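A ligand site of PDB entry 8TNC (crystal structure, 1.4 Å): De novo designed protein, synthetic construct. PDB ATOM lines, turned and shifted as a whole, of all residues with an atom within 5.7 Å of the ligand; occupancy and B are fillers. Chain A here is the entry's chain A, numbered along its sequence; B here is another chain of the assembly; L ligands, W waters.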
ATOM      1  N   TRP A  18       6.647   4.705   2.098  1.00  0.00           N
ATOM      2  CA  TRP A  18       7.581   4.139   1.125  1.00  0.00           C
ATOM      3  C   TRP A  18       8.902   4.906   1.143  1.00  0.00           C
ATOM      4  O   TRP A  18       9.994   4.309   1.136  1.00  0.00           O
ATOM      5  CB  TRP A  18       6.977   4.158  -0.276  1.00  0.00           C
ATOM      6  CG  TRP A  18       7.972   3.629  -1.280  1.00  0.00           C
ATOM      7  CD1 TRP A  18       8.473   4.294  -2.353  1.00  0.00           C
ATOM      8  CD2 TRP A  18       8.575   2.328  -1.284  1.00  0.00           C
ATOM      9  NE1 TRP A  18       9.377   3.500  -3.023  1.00  0.00           N
ATOM     10  CE2 TRP A  18       9.466   2.296  -2.381  1.00  0.00           C
ATOM     11  CE3 TRP A  18       8.482   1.205  -0.460  1.00  0.00           C
ATOM     12  CZ2 TRP A  18      10.243   1.173  -2.697  1.00  0.00           C
ATOM     13  CZ3 TRP A  18       9.258   0.073  -0.773  1.00  0.00           C
ATOM     14  CH2 TRP A  18      10.116   0.072  -1.883  1.00  0.00           C
ATOM     15  N   ILE A  21      10.744   3.779   4.163  1.00  0.00           N
ATOM     16  CA  ILE A  21      11.284   2.439   3.941  1.00  0.00           C
ATOM     17  C   ILE A  21      12.565   2.506   3.115  1.00  0.00           C
ATOM     18  O   ILE A  21      13.549   1.804   3.410  1.00  0.00           O
ATOM     19  CB  ILE A  21      10.222   1.551   3.274  1.00  0.00           C
ATOM     20  CG1 ILE A  21       9.129   1.233   4.299  1.00  0.00           C
ATOM     21  CG2 ILE A  21      10.846   0.274   2.705  1.00  0.00           C
ATOM     22  CD1 ILE A  21       7.797   0.807   3.682  1.00  0.00           C
ATOM     23  N   LEU A  24      15.202   3.579   5.476  1.00  0.00           N
ATOM     24  CA  LEU A  24      15.546   2.479   6.381  1.00  0.00           C
ATOM     25  C   LEU A  24      16.455   1.478   5.682  1.00  0.00           C
ATOM     26  O   LEU A  24      17.440   0.992   6.282  1.00  0.00           O
ATOM     27  CB  LEU A  24      14.266   1.794   6.887  1.00  0.00           C
ATOM     28  CG  LEU A  24      14.460   0.556   7.755  1.00  0.00           C
ATOM     29  CD1 LEU A  24      15.272   0.887   9.000  1.00  0.00           C
ATOM     30  CD2 LEU A  24      13.095  -0.049   8.133  1.00  0.00           C
ATOM     31  N   ALA A  25      16.112   1.123   4.437  1.00  0.00           N
ATOM     32  CA  ALA A  25      16.949   0.197   3.675  1.00  0.00           C
ATOM     33  C   ALA A  25      18.348   0.754   3.482  1.00  0.00           C
ATOM     34  O   ALA A  25      19.339   0.028   3.614  1.00  0.00           O
ATOM     35  CB  ALA A  25      16.314  -0.081   2.316  1.00  0.00           C
ATOM     36  N   THR A  28      20.296   0.654   6.845  1.00  0.00           N
ATOM     37  CA  THR A  28      20.717  -0.697   7.197  1.00  0.00           C
ATOM     38  C   THR A  28      21.812  -1.217   6.275  1.00  0.00           C
ATOM     39  O   THR A  28      22.715  -1.924   6.749  1.00  0.00           O
ATOM     40  CB  THR A  28      19.527  -1.629   7.324  1.00  0.00           C
ATOM     41  OG1 THR A  28      18.880  -1.688   6.079  1.00  0.00           O
ATOM     42  CG2 THR A  28      18.501  -1.124   8.337  1.00  0.00           C
ATOM     43  N   ASP A  29      21.818  -0.828   5.002  1.00  0.00           N
ATOM     44  CA  ASP A  29      22.945  -1.131   4.125  1.00  0.00           C
ATOM     45  C   ASP A  29      24.226  -0.516   4.684  1.00  0.00           C
ATOM     46  O   ASP A  29      25.279  -1.162   4.716  1.00  0.00           O
ATOM     47  CB  ASP A  29      22.700  -0.526   2.735  1.00  0.00           C
ATOM     48  CG  ASP A  29      21.806  -1.328   1.837  1.00  0.00           C
ATOM     49  OD1 ASP A  29      21.637  -2.506   2.111  1.00  0.00           O
ATOM     50  OD2 ASP A  29      21.297  -0.755   0.835  1.00  0.00           O
ATOM     51  N   GLU A  32      25.406  -2.426   7.724  1.00  0.00           N
ATOM     52  CA  GLU A  32      26.090  -3.663   7.329  1.00  0.00           C
ATOM     53  C   GLU A  32      27.529  -3.382   6.901  1.00  0.00           C
ATOM     54  O   GLU A  32      28.455  -4.130   7.273  1.00  0.00           O
ATOM     55  CB  GLU A  32      25.353  -4.332   6.176  1.00  0.00           C
ATOM     56  CG  GLU A  32      24.113  -5.046   6.591  1.00  0.00           C
ATOM     57  CD  GLU A  32      23.505  -5.887   5.475  1.00  0.00           C
ATOM     58  OE1 GLU A  32      23.827  -5.646   4.294  1.00  0.00           O
ATOM     59  OE2 GLU A  32      22.719  -6.792   5.803  1.00  0.00           O
ATOM     60  N   GLN A  54      12.778   3.154  11.487  1.00  0.00           N
ATOM     61  CA  GLN A  54      11.885   2.065  11.858  1.00  0.00           C
ATOM     62  C   GLN A  54      10.749   2.568  12.737  1.00  0.00           C
ATOM     63  O   GLN A  54       9.599   2.138  12.578  1.00  0.00           O
ATOM     64  CB  GLN A  54      12.724   1.009  12.596  1.00  0.00           C
ATOM     65  CG  GLN A  54      11.902  -0.225  13.041  1.00  0.00           C
ATOM     66  CD  GLN A  54      11.356  -1.004  11.874  1.00  0.00           C
ATOM     67  OE1 GLN A  54      12.066  -1.775  11.247  1.00  0.00           O
ATOM     68  NE2 GLN A  54      10.072  -0.806  11.547  1.00  0.00           N
ATOM     69  N   VAL A  57       8.229   4.123  10.442  1.00  0.00           N
ATOM     70  CA  VAL A  57       7.441   3.102   9.743  1.00  0.00           C
ATOM     71  C   VAL A  57       6.390   2.514  10.671  1.00  0.00           C
ATOM     72  O   VAL A  57       5.234   2.322  10.269  1.00  0.00           O
ATOM     73  CB  VAL A  57       8.335   1.999   9.123  1.00  0.00           C
ATOM     74  CG1 VAL A  57       7.467   0.928   8.402  1.00  0.00           C
ATOM     75  CG2 VAL A  57       9.343   2.617   8.134  1.00  0.00           C
ATOM     76  N   ASP A  58       6.747   2.231  11.915  1.00  0.00           N
ATOM     77  CA  ASP A  58       5.801   1.752  12.907  1.00  0.00           C
ATOM     78  C   ASP A  58       4.615   2.711  13.015  1.00  0.00           C
ATOM     79  O   ASP A  58       3.459   2.288  12.957  1.00  0.00           O
ATOM     80  CB  ASP A  58       6.448   1.632  14.300  1.00  0.00           C
ATOM     81  CG  ASP A  58       7.701   0.743  14.402  1.00  0.00           C
ATOM     82  OD1 ASP A  58       7.960  -0.126  13.562  1.00  0.00           O
ATOM     83  OD2 ASP A  58       8.433   0.918  15.417  1.00  0.00           O
ATOM     84  N   LEU A  90       0.723  -6.686   8.225  1.00  0.00           N
ATOM     85  CA  LEU A  90       1.859  -5.793   8.010  1.00  0.00           C
ATOM     86  C   LEU A  90       2.289  -5.150   9.320  1.00  0.00           C
ATOM     87  O   LEU A  90       3.479  -5.146   9.656  1.00  0.00           O
ATOM     88  CB  LEU A  90       1.505  -4.749   6.968  1.00  0.00           C
ATOM     89  CG  LEU A  90       2.526  -3.637   6.739  1.00  0.00           C
ATOM     90  CD1 LEU A  90       3.884  -4.144   6.175  1.00  0.00           C
ATOM     91  CD2 LEU A  90       1.877  -2.565   5.830  1.00  0.00           C
ATOM     92  N   THR A  93       4.169  -7.540  11.565  1.00  0.00           N
ATOM     93  CA  THR A  93       5.504  -7.823  11.049  1.00  0.00           C
ATOM     94  C   THR A  93       6.447  -6.630  11.284  1.00  0.00           C
ATOM     95  O   THR A  93       7.613  -6.800  11.704  1.00  0.00           O
ATOM     96  CB  THR A  93       5.411  -8.157   9.560  1.00  0.00           C
ATOM     97  OG1 THR A  93       4.491  -9.248   9.362  1.00  0.00           O
ATOM     98  CG2 THR A  93       6.769  -8.559   8.999  1.00  0.00           C
ATOM     99  N   VAL A  94       5.937  -5.416  11.044  1.00  0.00           N
ATOM    100  CA  VAL A  94       6.681  -4.188  11.327  1.00  0.00           C
ATOM    101  C   VAL A  94       7.094  -4.116  12.791  1.00  0.00           C
ATOM    102  O   VAL A  94       8.250  -3.780  13.112  1.00  0.00           O
ATOM    103  CB  VAL A  94       5.831  -2.960  10.913  1.00  0.00           C
ATOM    104  CG1 VAL A  94       6.426  -1.698  11.453  1.00  0.00           C
ATOM    105  CG2 VAL A  94       5.726  -2.893   9.403  1.00  0.00           C
ATOM    106  N   ALA A  97       9.843  -6.585  13.403  1.00  0.00           N
ATOM    107  CA  ALA A  97      11.087  -6.003  12.889  1.00  0.00           C
ATOM    108  C   ALA A  97      11.613  -4.952  13.857  1.00  0.00           C
ATOM    109  O   ALA A  97      12.820  -4.894  14.133  1.00  0.00           O
ATOM    110  CB  ALA A  97      10.872  -5.398  11.511  1.00  0.00           C
ATOM    111  N   PHE A 120      20.300  -8.906  13.996  1.00  0.00           N
ATOM    112  CA  PHE A 120      20.342  -8.161  12.745  1.00  0.00           C
ATOM    113  C   PHE A 120      19.877  -9.025  11.569  1.00  0.00           C
ATOM    114  O   PHE A 120      19.104  -8.580  10.716  1.00  0.00           O
ATOM    115  CB  PHE A 120      21.717  -7.550  12.511  1.00  0.00           C
ATOM    116  CG  PHE A 120      21.715  -6.486  11.463  1.00  0.00           C
ATOM    117  CD1 PHE A 120      21.891  -6.820  10.136  1.00  0.00           C
ATOM    118  CD2 PHE A 120      21.453  -5.160  11.791  1.00  0.00           C
ATOM    119  CE1 PHE A 120      21.875  -5.842   9.148  1.00  0.00           C
ATOM    120  CE2 PHE A 120      21.437  -4.189  10.819  1.00  0.00           C
ATOM    121  CZ  PHE A 120      21.641  -4.532   9.506  1.00  0.00           C
ATOM    122  N   PHE A 123      16.181  -9.334  11.684  1.00  0.00           N
ATOM    123  CA  PHE A 123      15.583  -8.080  11.244  1.00  0.00           C
ATOM    124  C   PHE A 123      15.496  -8.037   9.731  1.00  0.00           C
ATOM    125  O   PHE A 123      14.464  -7.659   9.172  1.00  0.00           O
ATOM    126  CB  PHE A 123      16.377  -6.882  11.787  1.00  0.00           C
ATOM    127  CG  PHE A 123      16.082  -5.616  11.056  1.00  0.00           C
ATOM    128  CD1 PHE A 123      14.930  -4.865  11.338  1.00  0.00           C
ATOM    129  CD2 PHE A 123      16.920  -5.182  10.043  1.00  0.00           C
ATOM    130  CE1 PHE A 123      14.676  -3.693  10.662  1.00  0.00           C
ATOM    131  CE2 PHE A 123      16.643  -4.012   9.349  1.00  0.00           C
ATOM    132  CZ  PHE A 123      15.506  -3.276   9.662  1.00  0.00           C
ATOM    133  N   VAL A 124      16.573  -8.440   9.039  1.00  0.00           N
ATOM    134  CA  VAL A 124      16.561  -8.402   7.578  1.00  0.00           C
ATOM    135  C   VAL A 124      15.443  -9.287   7.012  1.00  0.00           C
ATOM    136  O   VAL A 124      14.728  -8.901   6.079  1.00  0.00           O
ATOM    137  CB  VAL A 124      17.944  -8.776   7.015  1.00  0.00           C
ATOM    138  CG1 VAL A 124      17.869  -8.963   5.501  1.00  0.00           C
ATOM    139  CG2 VAL A 124      18.960  -7.715   7.415  1.00  0.00           C
ATOM    140  N   LEU A 126      12.680 -10.183   8.498  1.00  0.00           N
ATOM    141  CA  LEU A 126      11.390  -9.559   8.790  1.00  0.00           C
ATOM    142  C   LEU A 126      11.136  -8.374   7.891  1.00  0.00           C
ATOM    143  O   LEU A 126       9.999  -8.142   7.446  1.00  0.00           O
ATOM    144  CB  LEU A 126      11.357  -9.141  10.264  1.00  0.00           C
ATOM    145  CG  LEU A 126      11.207 -10.296  11.256  1.00  0.00           C
ATOM    146  CD1 LEU A 126      11.580  -9.867  12.677  1.00  0.00           C
ATOM    147  CD2 LEU A 126       9.776 -10.864  11.236  1.00  0.00           C
ATOM    148  N   GLY A 127      12.162  -7.577   7.617  1.00  0.00           N
ATOM    149  CA  GLY A 127      12.016  -6.477   6.678  1.00  0.00           C
ATOM    150  C   GLY A 127      11.562  -6.939   5.296  1.00  0.00           C
ATOM    151  O   GLY A 127      10.685  -6.320   4.658  1.00  0.00           O
ATOM    152  N   ASN A 128      12.167  -8.020   4.789  1.00  0.00           N
ATOM    153  CA  ASN A 128      11.741  -8.536   3.491  1.00  0.00           C
ATOM    154  C   ASN A 128      10.314  -9.064   3.540  1.00  0.00           C
ATOM    155  O   ASN A 128       9.553  -8.893   2.564  1.00  0.00           O
ATOM    156  CB  ASN A 128      12.730  -9.606   3.036  1.00  0.00           C
ATOM    157  CG  ASN A 128      14.034  -9.008   2.527  1.00  0.00           C
ATOM    158  OD1 ASN A 128      14.031  -7.991   1.850  1.00  0.00           O
ATOM    159  ND2 ASN A 128      15.140  -9.661   2.826  1.00  0.00           N
ATOM    160  N   ALA A 130       7.955  -7.865   5.522  1.00  0.00           N
ATOM    161  CA  ALA A 130       7.116  -6.685   5.559  1.00  0.00           C
ATOM    162  C   ALA A 130       6.990  -6.049   4.178  1.00  0.00           C
ATOM    163  O   ALA A 130       5.917  -5.543   3.810  1.00  0.00           O
ATOM    164  CB  ALA A 130       7.707  -5.709   6.583  1.00  0.00           C
ATOM    165  N   ASP A 131       8.069  -6.073   3.388  1.00  0.00           N
ATOM    166  CA  ASP A 131       7.995  -5.540   2.036  1.00  0.00           C
ATOM    167  C   ASP A 131       6.961  -6.291   1.191  1.00  0.00           C
ATOM    168  O   ASP A 131       6.192  -5.669   0.453  1.00  0.00           O
ATOM    169  CB  ASP A 131       9.367  -5.583   1.382  1.00  0.00           C
ATOM    170  CG  ASP A 131       9.384  -4.943  -0.001  1.00  0.00           C
ATOM    171  OD1 ASP A 131       9.526  -3.705  -0.060  1.00  0.00           O
ATOM    172  OD2 ASP A 131       9.279  -5.671  -1.015  1.00  0.00           O
ATOM    173  N   PHE A 134       3.581  -5.024   2.353  1.00  0.00           N
ATOM    174  CA  PHE A 134       3.364  -3.649   1.908  1.00  0.00           C
ATOM    175  C   PHE A 134       2.924  -3.603   0.447  1.00  0.00           C
ATOM    176  O   PHE A 134       1.961  -2.918   0.095  1.00  0.00           O
ATOM    177  CB  PHE A 134       4.664  -2.856   2.091  1.00  0.00           C
ATOM    178  CG  PHE A 134       4.532  -1.404   1.896  1.00  0.00           C
ATOM    179  CD1 PHE A 134       4.150  -0.601   2.942  1.00  0.00           C
ATOM    180  CD2 PHE A 134       4.791  -0.804   0.667  1.00  0.00           C
ATOM    181  CE1 PHE A 134       4.009   0.769   2.784  1.00  0.00           C
ATOM    182  CE2 PHE A 134       4.656   0.554   0.504  1.00  0.00           C
ATOM    183  CZ  PHE A 134       4.259   1.343   1.570  1.00  0.00           C
ATOM    184  N   LYS B  33      23.735   2.439  -5.918  1.00  0.00           N
ATOM    185  CA  LYS B  33      23.137   1.121  -6.085  1.00  0.00           C
ATOM    186  C   LYS B  33      21.898   1.189  -6.955  1.00  0.00           C
ATOM    187  O   LYS B  33      21.722   0.355  -7.853  1.00  0.00           O
ATOM    188  CB  LYS B  33      22.822   0.549  -4.696  1.00  0.00           C
ATOM    189  CG  LYS B  33      22.280  -0.867  -4.696  1.00  0.00           C
ATOM    190  CD  LYS B  33      22.014  -1.312  -3.242  1.00  0.00           C
ATOM    191  CE  LYS B  33      21.169  -2.571  -3.177  1.00  0.00           C
ATOM    192  NZ  LYS B  33      21.177  -3.129  -1.789  1.00  0.00           N
HETATM  193  C1  LIG L   1      18.500  -5.180   5.160  1.00  0.00           C
HETATM  194  C2  LIG L   1      19.918  -4.601   5.179  1.00  0.00           C
HETATM  195  C3  LIG L   1      20.678  -4.546   3.883  1.00  0.00           C
HETATM  196  N1  LIG L   1      19.793  -4.324   2.687  1.00  0.00           N
HETATM  197  C4  LIG L   1      18.483  -3.746   3.073  1.00  0.00           C
HETATM  198  C5  LIG L   1      17.736  -4.818   3.880  1.00  0.00           C
HETATM  199  C6  LIG L   1      16.293  -4.394   4.099  1.00  0.00           C
HETATM  200  C7  LIG L   1      15.931  -3.435   5.037  1.00  0.00           C
HETATM  201  C8  LIG L   1      14.612  -3.069   5.207  1.00  0.00           C
HETATM  202  C9  LIG L   1      15.292  -5.007   3.356  1.00  0.00           C
HETATM  203  C10 LIG L   1      13.962  -4.677   3.543  1.00  0.00           C
HETATM  204  C11 LIG L   1      13.630  -3.696   4.458  1.00  0.00           C
HETATM  205  N2  LIG L   1      12.261  -3.347   4.660  1.00  0.00           N
HETATM  206  C12 LIG L   1      11.282  -3.236   3.751  1.00  0.00           C
HETATM  207  N3  LIG L   1      11.854  -3.106   5.932  1.00  0.00           N
HETATM  208  C13 LIG L   1      10.530  -2.830   5.803  1.00  0.00           C
HETATM  209  C14 LIG L   1      10.141  -2.886   4.449  1.00  0.00           C
HETATM  210  C15 LIG L   1       8.799  -2.627   4.092  1.00  0.00           C
HETATM  211  C16 LIG L   1       7.903  -2.311   5.081  1.00  0.00           C
HETATM  212  C17 LIG L   1       8.293  -2.239   6.415  1.00  0.00           C
HETATM  213  C18 LIG L   1       9.604  -2.491   6.826  1.00  0.00           C
HETATM  214  C19 LIG L   1       9.959  -2.425   8.282  1.00  0.00           C
HETATM  215  O1  LIG L   1       9.095  -2.110   9.122  1.00  0.00           O
HETATM  216  N4  LIG L   1      11.172  -2.800   8.654  1.00  0.00           N
HETATM  217  O   HOH W   1      19.911  -7.277   2.407  1.00  0.00           O
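The side-chain carboxylate (OD1) of Asp 29 lies within salt-bridge range of a nitrogen (N1) of the ligand (2.7 Å).
NE2 of Gln 54 lies within hydrogen-bond range of O1 of the ligand (2.9 Å).
The side-chain amino group (NZ) of Lys 33 of chain B is in salt-bridge range of the side-chain carboxylate (OD2) of Asp 29 (3.5 Å).
The side-chain amide nitrogen (NE2) of Gln 54 is in hydrogen-bond range of the side-chain carboxylate (OD1) of Asp 58, 3.0 Å away.
The side-chain hydroxyl (OG1) of Thr 28 is in hydrogen-bond range of the backbone carbonyl oxygen (O) of Leu 24, 3.0 Å away.
The side-chain hydroxyl (OG1) of Thr 28 is in hydrogen-bond range of the backbone carbonyl oxygen (O) of Ala 25 (3.0 Å).
ND2 of Asn 128 sits at hydrogen-bond distance from O of Val 124 (3.4 Å).
N2 of the ligand lies close to O of Gly 127 (3.4 Å).
Ile 21 touches the ligand (CD1 to C16, 3.4 Å).
Leu 24 touches the ligand (CD2 to N4, 3.4 Å).
Ala 25 touches the ligand (O to C4, 3.9 Å).
Thr 28 touches the ligand (OG1 to C2, 3.2 Å).
OE1 of Glu 32 touches C3 of the ligand, at 3.4 Å.
Val 57 touches the ligand.
Val 94 touches the ligand.
CB of Ala 97 touches N4 of the ligand, 3.9 Å away.
CG2 of Val 124 touches C1 of the ligand, 3.4 Å away.
Asn 128 touches the ligand.
Ala 130 touches the ligand (CB to C17, 3.5 Å).
Asp 131 touches the ligand.
Hydrophobic or aromatic side chains within 4 Å of the ligand: Ile 21, Leu 24, Val 57, Val 94, Ala 97, Val 124 and Ala 130.
15 residues have an atom within 4 Å of the ligand: Ile 21, Leu 24, Ala 25, Thr 28, Asp 29, Glu 32, Gln 54, Val 57, Val 94, Ala 97, Val 124, Gly 127, Asn 128, Ala 130 and Asp 131.
The nearest printed residue that does not touch the ligand is Phe 123 (4.1 Å).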
